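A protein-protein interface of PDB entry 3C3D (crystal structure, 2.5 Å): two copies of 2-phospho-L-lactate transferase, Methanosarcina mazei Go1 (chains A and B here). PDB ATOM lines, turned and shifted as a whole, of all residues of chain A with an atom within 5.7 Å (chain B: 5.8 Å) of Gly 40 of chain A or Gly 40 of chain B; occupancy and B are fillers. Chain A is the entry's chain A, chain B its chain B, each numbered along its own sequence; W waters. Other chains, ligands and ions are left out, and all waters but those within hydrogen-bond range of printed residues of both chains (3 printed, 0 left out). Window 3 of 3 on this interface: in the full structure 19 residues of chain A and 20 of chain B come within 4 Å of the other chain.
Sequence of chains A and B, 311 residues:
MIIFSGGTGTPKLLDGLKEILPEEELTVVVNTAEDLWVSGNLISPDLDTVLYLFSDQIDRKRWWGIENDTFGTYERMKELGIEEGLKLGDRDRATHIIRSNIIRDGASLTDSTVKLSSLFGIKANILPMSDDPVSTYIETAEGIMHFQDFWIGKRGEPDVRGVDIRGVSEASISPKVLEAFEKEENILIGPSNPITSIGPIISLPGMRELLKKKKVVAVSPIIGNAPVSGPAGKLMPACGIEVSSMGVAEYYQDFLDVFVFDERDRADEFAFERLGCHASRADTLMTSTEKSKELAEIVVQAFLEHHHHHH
The backbone carbonyl oxygen of Ser 39 of chain A lies within hydrogen-bond range of the side-chain amide nitrogen of Asn 41 of chain B (3.1 Å).
ND2 of Asn 41 of chain A is in hydrogen-bond range of O of Ser 39 of chain B (3.0 Å).
N of Gly 40 of chain A sits close to NH2 of Arg 104 of chain B (3.2 Å).
NH2 of Arg 104 of chain A lies close to N of Gly 40 of chain B, 3.2 Å away.
CA of Ser 39 of chain A touches OD1 of Asn 101 of chain B (3.7 Å).
Ser 39 of chain A touches Arg 104 of chain B.
Gly 40 of chain B touches Gly 40 of chain A (CA to O, 3.5 Å).
Gly 40 of chain A touches Asn 41 of chain B.
Ser 39 of chain B touches Asn 101 of chain A (CA to OD1, 3.97 Å).
Ser 39 of chain B touches Arg 104 of chain A.
Water W3 bridges the backbone NH (N) of Ser 39 of chain A and the side-chain amide oxygen (OD1) of Asn 101 of chain B.
Water W1 lies within hydrogen-bond range of OG of Ser 39 of chain A (3.0 Å) and ND2 of Asn 101 of chain B (3.3 Å).
Water W2 lies within hydrogen-bond range of the backbone NH of Ser 39 of chain B and the side-chain amide oxygen of Asn 101 of chain A.
Val 38 of chain A touches none of the printed residues of chain B.
Of the printed residues of chain B, Gly 40 of chain A touches Gly 40 (3.5 Å), Asn 41 (3.999 Å) and Arg 104 (3.2 Å).
Printed residues of chain B within 4 Å of Asn 41 of chain A: Ser 39.
Of the printed residues of chain B, Asn 101 of chain A touches Ser 39 (3.97 Å).
Printed residues of chain B within 4 Å of Arg 104 of chain A: Ser 39 and Gly 40.
Gly 40 of chain B touches just these residues of chain A: Gly 40 and Arg 104.
Printed residues of chain A within 4 Å of Arg 104 of chain B: Ser 39 (3.4 Å) and Gly 40 (3.2 Å).
Of the 9 printed residues of chain A, 5 touch a printed residue of chain B.
Of the 9 printed residues of chain B, 5 touch a printed residue of chain A.
Among the printed residues, 10 pairs touch across the chains.
Among the printed residues, no Asp or Glu carboxylate lies within 4 Å of a Lys or Arg side-chain nitrogen of the other chain.
O of Gly 40 of chain A sits at hydrogen-bond distance from NH1 of Arg 104 of chain A, 3.0 Å away.
NH2 of Arg 104 of chain A is in hydrogen-bond range of OD1 of Asn 41 of chain A.
The side-chain amide oxygen of Asn 101 of chain A sits at hydrogen-bond distance from the guanidinium group of Arg 104 of chain A (2.9 Å).
The backbone carbonyl oxygen of Gly 40 of chain B sits at hydrogen-bond distance from the guanidinium group of Arg 104 of chain B.
The side-chain amide oxygen (OD1) of Asn 41 of chain B is in hydrogen-bond range of the guanidinium group (NH2) of Arg 104 of chain B.
The guanidinium group of Arg 104 of chain B is in hydrogen-bond range of the side-chain amide oxygen of Asn 101 of chain B, at 2.7 Å.
Ser 39 of chain A touches Asn 41 of chain B, and with the chains exchanged Asn 41 of chain A touches Ser 39 of chain B.
Ser 39 of chain A touches Asn 101 of chain B, and with the chains exchanged Asn 101 of chain A touches Ser 39 of chain B.
Ser 39 of chain A touches Arg 104 of chain B, and with the chains exchanged Arg 104 of chain A touches Ser 39 of chain B.
Gly 40 of chain A touches Asn 41 of chain B, but with the chains exchanged Asn 41 of chain A does not touch Gly 40 of chain B (4.03 Å).
Of the 10 pairs that touch across the chains among the printed residues, 9 have their exchanged pair printed and touching as well.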
ATOM      1  N   TRP A  37      30.944 -13.815 -38.811  1.00  0.00           N
ATOM      2  CA  TRP A  37      30.817 -13.677 -37.375  1.00  0.00           C
ATOM      3  C   TRP A  37      32.137 -13.025 -36.986  1.00  0.00           C
ATOM      4  O   TRP A  37      33.206 -13.525 -37.334  1.00  0.00           O
ATOM      5  CB  TRP A  37      30.675 -15.026 -36.703  1.00  0.00           C
ATOM      6  CG  TRP A  37      29.347 -15.624 -36.927  1.00  0.00           C
ATOM      7  CD1 TRP A  37      28.927 -16.304 -38.036  1.00  0.00           C
ATOM      8  CD2 TRP A  37      28.221 -15.538 -36.056  1.00  0.00           C
ATOM      9  NE1 TRP A  37      27.596 -16.642 -37.907  1.00  0.00           N
ATOM     10  CE2 TRP A  37      27.139 -16.181 -36.701  1.00  0.00           C
ATOM     11  CE3 TRP A  37      28.018 -14.975 -34.792  1.00  0.00           C
ATOM     12  CZ2 TRP A  37      25.871 -16.278 -36.123  1.00  0.00           C
ATOM     13  CZ3 TRP A  37      26.759 -15.070 -34.214  1.00  0.00           C
ATOM     14  CH2 TRP A  37      25.697 -15.719 -34.884  1.00  0.00           C
ATOM     15  N   VAL A  38      32.066 -11.884 -36.313  1.00  0.00           N
ATOM     16  CA  VAL A  38      33.260 -11.163 -35.896  1.00  0.00           C
ATOM     17  C   VAL A  38      33.113 -10.797 -34.427  1.00  0.00           C
ATOM     18  O   VAL A  38      32.093 -10.230 -34.017  1.00  0.00           O
ATOM     19  CB  VAL A  38      33.445  -9.861 -36.700  1.00  0.00           C
ATOM     20  CG1 VAL A  38      34.692  -9.115 -36.220  1.00  0.00           C
ATOM     21  CG2 VAL A  38      33.555 -10.174 -38.177  1.00  0.00           C
ATOM     22  N   SER A  39      34.120 -11.136 -33.628  1.00  0.00           N
ATOM     23  CA  SER A  39      34.076 -10.826 -32.214  1.00  0.00           C
ATOM     24  C   SER A  39      32.797 -11.312 -31.534  1.00  0.00           C
ATOM     25  O   SER A  39      32.181 -10.577 -30.770  1.00  0.00           O
ATOM     26  CB  SER A  39      34.215  -9.324 -32.012  1.00  0.00           C
ATOM     27  OG  SER A  39      35.437  -8.873 -32.563  1.00  0.00           O
ATOM     28  N   GLY A  40      32.398 -12.545 -31.841  1.00  0.00           N
ATOM     29  CA  GLY A  40      31.220 -13.136 -31.223  1.00  0.00           C
ATOM     30  C   GLY A  40      29.865 -12.803 -31.812  1.00  0.00           C
ATOM     31  O   GLY A  40      28.841 -13.331 -31.357  1.00  0.00           O
ATOM     32  N   ASN A  41      29.829 -11.956 -32.832  1.00  0.00           N
ATOM     33  CA  ASN A  41      28.541 -11.582 -33.389  1.00  0.00           C
ATOM     34  C   ASN A  41      28.516 -11.476 -34.900  1.00  0.00           C
ATOM     35  O   ASN A  41      29.490 -11.071 -35.527  1.00  0.00           O
ATOM     36  CB  ASN A  41      28.082 -10.273 -32.746  1.00  0.00           C
ATOM     37  CG  ASN A  41      27.849 -10.422 -31.258  1.00  0.00           C
ATOM     38  OD1 ASN A  41      26.903 -11.084 -30.834  1.00  0.00           O
ATOM     39  ND2 ASN A  41      28.721  -9.824 -30.454  1.00  0.00           N
ATOM     40  N   LEU A  42      27.378 -11.836 -35.476  1.00  0.00           N
ATOM     41  CA  LEU A  42      27.229 -11.822 -36.915  1.00  0.00           C
ATOM     42  C   LEU A  42      27.155 -10.445 -37.558  1.00  0.00           C
ATOM     43  O   LEU A  42      26.341  -9.610 -37.193  1.00  0.00           O
ATOM     44  CB  LEU A  42      25.995 -12.621 -37.311  1.00  0.00           C
ATOM     45  CG  LEU A  42      25.692 -12.745 -38.804  1.00  0.00           C
ATOM     46  CD1 LEU A  42      26.879 -13.397 -39.547  1.00  0.00           C
ATOM     47  CD2 LEU A  42      24.436 -13.583 -38.961  1.00  0.00           C
ATOM     48  N   SER A 100      22.397 -11.263 -33.422  1.00  0.00           N
ATOM     49  CA  SER A 100      22.984 -12.526 -32.990  1.00  0.00           C
ATOM     50  C   SER A 100      22.275 -13.174 -31.794  1.00  0.00           C
ATOM     51  O   SER A 100      22.212 -14.405 -31.697  1.00  0.00           O
ATOM     52  CB  SER A 100      24.481 -12.332 -32.730  1.00  0.00           C
ATOM     53  OG  SER A 100      25.098 -11.741 -33.866  1.00  0.00           O
ATOM     54  N   ASN A 101      21.735 -12.370 -30.884  1.00  0.00           N
ATOM     55  CA  ASN A 101      21.019 -12.980 -29.768  1.00  0.00           C
ATOM     56  C   ASN A 101      19.822 -13.724 -30.329  1.00  0.00           C
ATOM     57  O   ASN A 101      19.490 -14.820 -29.874  1.00  0.00           O
ATOM     58  CB  ASN A 101      20.561 -11.933 -28.750  1.00  0.00           C
ATOM     59  CG  ASN A 101      21.711 -11.411 -27.902  1.00  0.00           C
ATOM     60  OD1 ASN A 101      22.739 -12.096 -27.729  1.00  0.00           O
ATOM     61  ND2 ASN A 101      21.547 -10.200 -27.362  1.00  0.00           N
ATOM     62  N   ARG A 104      21.060 -16.872 -31.948  1.00  0.00           N
ATOM     63  CA  ARG A 104      21.484 -17.781 -30.898  1.00  0.00           C
ATOM     64  C   ARG A 104      20.286 -18.443 -30.223  1.00  0.00           C
ATOM     65  O   ARG A 104      20.386 -19.578 -29.759  1.00  0.00           O
ATOM     66  CB  ARG A 104      22.336 -17.044 -29.859  1.00  0.00           C
ATOM     67  CG  ARG A 104      23.795 -16.908 -30.261  1.00  0.00           C
ATOM     68  CD  ARG A 104      24.625 -16.356 -29.119  1.00  0.00           C
ATOM     69  NE  ARG A 104      24.486 -14.909 -28.959  1.00  0.00           N
ATOM     70  CZ  ARG A 104      25.303 -14.024 -29.517  1.00  0.00           C
ATOM     71  NH1 ARG A 104      26.313 -14.445 -30.275  1.00  0.00           N
ATOM     72  NH2 ARG A 104      25.125 -12.724 -29.298  1.00  0.00           N
ATOM     73  N   TRP B  37      28.198 -16.233 -20.785  1.00  0.00           N
ATOM     74  CA  TRP B  37      28.379 -15.713 -22.130  1.00  0.00           C
ATOM     75  C   TRP B  37      27.262 -14.688 -22.279  1.00  0.00           C
ATOM     76  O   TRP B  37      26.101 -14.990 -22.013  1.00  0.00           O
ATOM     77  CB  TRP B  37      28.233 -16.807 -23.171  1.00  0.00           C
ATOM     78  CG  TRP B  37      29.397 -17.720 -23.220  1.00  0.00           C
ATOM     79  CD1 TRP B  37      29.649 -18.776 -22.387  1.00  0.00           C
ATOM     80  CD2 TRP B  37      30.508 -17.641 -24.121  1.00  0.00           C
ATOM     81  NE1 TRP B  37      30.852 -19.359 -22.718  1.00  0.00           N
ATOM     82  CE2 TRP B  37      31.402 -18.684 -23.775  1.00  0.00           C
ATOM     83  CE3 TRP B  37      30.837 -16.791 -25.183  1.00  0.00           C
ATOM     84  CZ2 TRP B  37      32.602 -18.898 -24.455  1.00  0.00           C
ATOM     85  CZ3 TRP B  37      32.029 -17.003 -25.865  1.00  0.00           C
ATOM     86  CH2 TRP B  37      32.900 -18.050 -25.498  1.00  0.00           C
ATOM     87  N   VAL B  38      27.625 -13.467 -22.644  1.00  0.00           N
ATOM     88  CA  VAL B  38      26.652 -12.393 -22.800  1.00  0.00           C
ATOM     89  C   VAL B  38      26.983 -11.633 -24.072  1.00  0.00           C
ATOM     90  O   VAL B  38      28.114 -11.191 -24.256  1.00  0.00           O
ATOM     91  CB  VAL B  38      26.709 -11.397 -21.620  1.00  0.00           C
ATOM     92  CG1 VAL B  38      25.635 -10.323 -21.783  1.00  0.00           C
ATOM     93  CG2 VAL B  38      26.529 -12.133 -20.320  1.00  0.00           C
ATOM     94  N   SER B  39      25.990 -11.495 -24.944  1.00  0.00           N
ATOM     95  CA  SER B  39      26.160 -10.792 -26.202  1.00  0.00           C
ATOM     96  C   SER B  39      27.296 -11.367 -27.050  1.00  0.00           C
ATOM     97  O   SER B  39      28.077 -10.639 -27.656  1.00  0.00           O
ATOM     98  CB  SER B  39      26.367  -9.308 -25.932  1.00  0.00           C
ATOM     99  OG  SER B  39      25.248  -8.800 -25.220  1.00  0.00           O
ATOM    100  N   GLY B  40      27.368 -12.693 -27.067  1.00  0.00           N
ATOM    101  CA  GLY B  40      28.362 -13.380 -27.859  1.00  0.00           C
ATOM    102  C   GLY B  40      29.736 -13.512 -27.248  1.00  0.00           C
ATOM    103  O   GLY B  40      30.620 -14.122 -27.859  1.00  0.00           O
ATOM    104  N   ASN B  41      29.940 -12.960 -26.055  1.00  0.00           N
ATOM    105  CA  ASN B  41      31.257 -13.062 -25.452  1.00  0.00           C
ATOM    106  C   ASN B  41      31.289 -13.461 -23.995  1.00  0.00           C
ATOM    107  O   ASN B  41      30.408 -13.113 -23.210  1.00  0.00           O
ATOM    108  CB  ASN B  41      32.022 -11.773 -25.688  1.00  0.00           C
ATOM    109  CG  ASN B  41      32.313 -11.549 -27.160  1.00  0.00           C
ATOM    110  OD1 ASN B  41      33.066 -12.310 -27.773  1.00  0.00           O
ATOM    111  ND2 ASN B  41      31.706 -10.509 -27.740  1.00  0.00           N
ATOM    112  N   LEU B  42      32.318 -14.223 -23.647  1.00  0.00           N
ATOM    113  CA  LEU B  42      32.471 -14.713 -22.289  1.00  0.00           C
ATOM    114  C   LEU B  42      32.830 -13.639 -21.271  1.00  0.00           C
ATOM    115  O   LEU B  42      33.787 -12.897 -21.453  1.00  0.00           O
ATOM    116  CB  LEU B  42      33.520 -15.816 -22.254  1.00  0.00           C
ATOM    117  CG  LEU B  42      33.736 -16.470 -20.892  1.00  0.00           C
ATOM    118  CD1 LEU B  42      32.412 -16.955 -20.306  1.00  0.00           C
ATOM    119  CD2 LEU B  42      34.706 -17.631 -21.075  1.00  0.00           C
ATOM    120  N   SER B 100      37.386 -14.223 -25.615  1.00  0.00           N
ATOM    121  CA  SER B 100      36.541 -15.123 -26.381  1.00  0.00           C
ATOM    122  C   SER B 100      37.092 -15.500 -27.755  1.00  0.00           C
ATOM    123  O   SER B 100      36.847 -16.605 -28.227  1.00  0.00           O
ATOM    124  CB  SER B 100      35.140 -14.530 -26.489  1.00  0.00           C
ATOM    125  OG  SER B 100      34.605 -14.315 -25.194  1.00  0.00           O
ATOM    126  N   ASN B 101      37.832 -14.605 -28.398  1.00  0.00           N
ATOM    127  CA  ASN B 101      38.418 -14.926 -29.703  1.00  0.00           C
ATOM    128  C   ASN B 101      39.471 -16.019 -29.481  1.00  0.00           C
ATOM    129  O   ASN B 101      39.641 -16.920 -30.304  1.00  0.00           O
ATOM    130  CB  ASN B 101      39.088 -13.692 -30.345  1.00  0.00           C
ATOM    131  CG  ASN B 101      38.087 -12.709 -30.931  1.00  0.00           C
ATOM    132  OD1 ASN B 101      36.898 -13.018 -31.086  1.00  0.00           O
ATOM    133  ND2 ASN B 101      38.568 -11.518 -31.275  1.00  0.00           N
ATOM    134  N   ARG B 104      37.592 -19.167 -28.964  1.00  0.00           N
ATOM    135  CA  ARG B 104      36.978 -19.626 -30.196  1.00  0.00           C
ATOM    136  C   ARG B 104      38.007 -20.282 -31.114  1.00  0.00           C
ATOM    137  O   ARG B 104      37.641 -21.025 -32.018  1.00  0.00           O
ATOM    138  CB  ARG B 104      36.279 -18.473 -30.928  1.00  0.00           C
ATOM    139  CG  ARG B 104      34.861 -18.182 -30.433  1.00  0.00           C
ATOM    140  CD  ARG B 104      34.215 -17.076 -31.262  1.00  0.00           C
ATOM    141  NE  ARG B 104      34.695 -15.726 -30.947  1.00  0.00           N
ATOM    142  CZ  ARG B 104      34.125 -14.917 -30.050  1.00  0.00           C
ATOM    143  NH1 ARG B 104      33.053 -15.325 -29.372  1.00  0.00           N
ATOM    144  NH2 ARG B 104      34.612 -13.690 -29.849  1.00  0.00           N
HETATM  145  O   HOH W   1      37.602 -10.171 -34.181  1.00  0.00           O
HETATM  146  O   HOH W   2      22.953 -12.217 -24.467  1.00  0.00           O
HETATM  147  O   HOH W   3      36.410 -12.502 -34.488  1.00  0.00           O
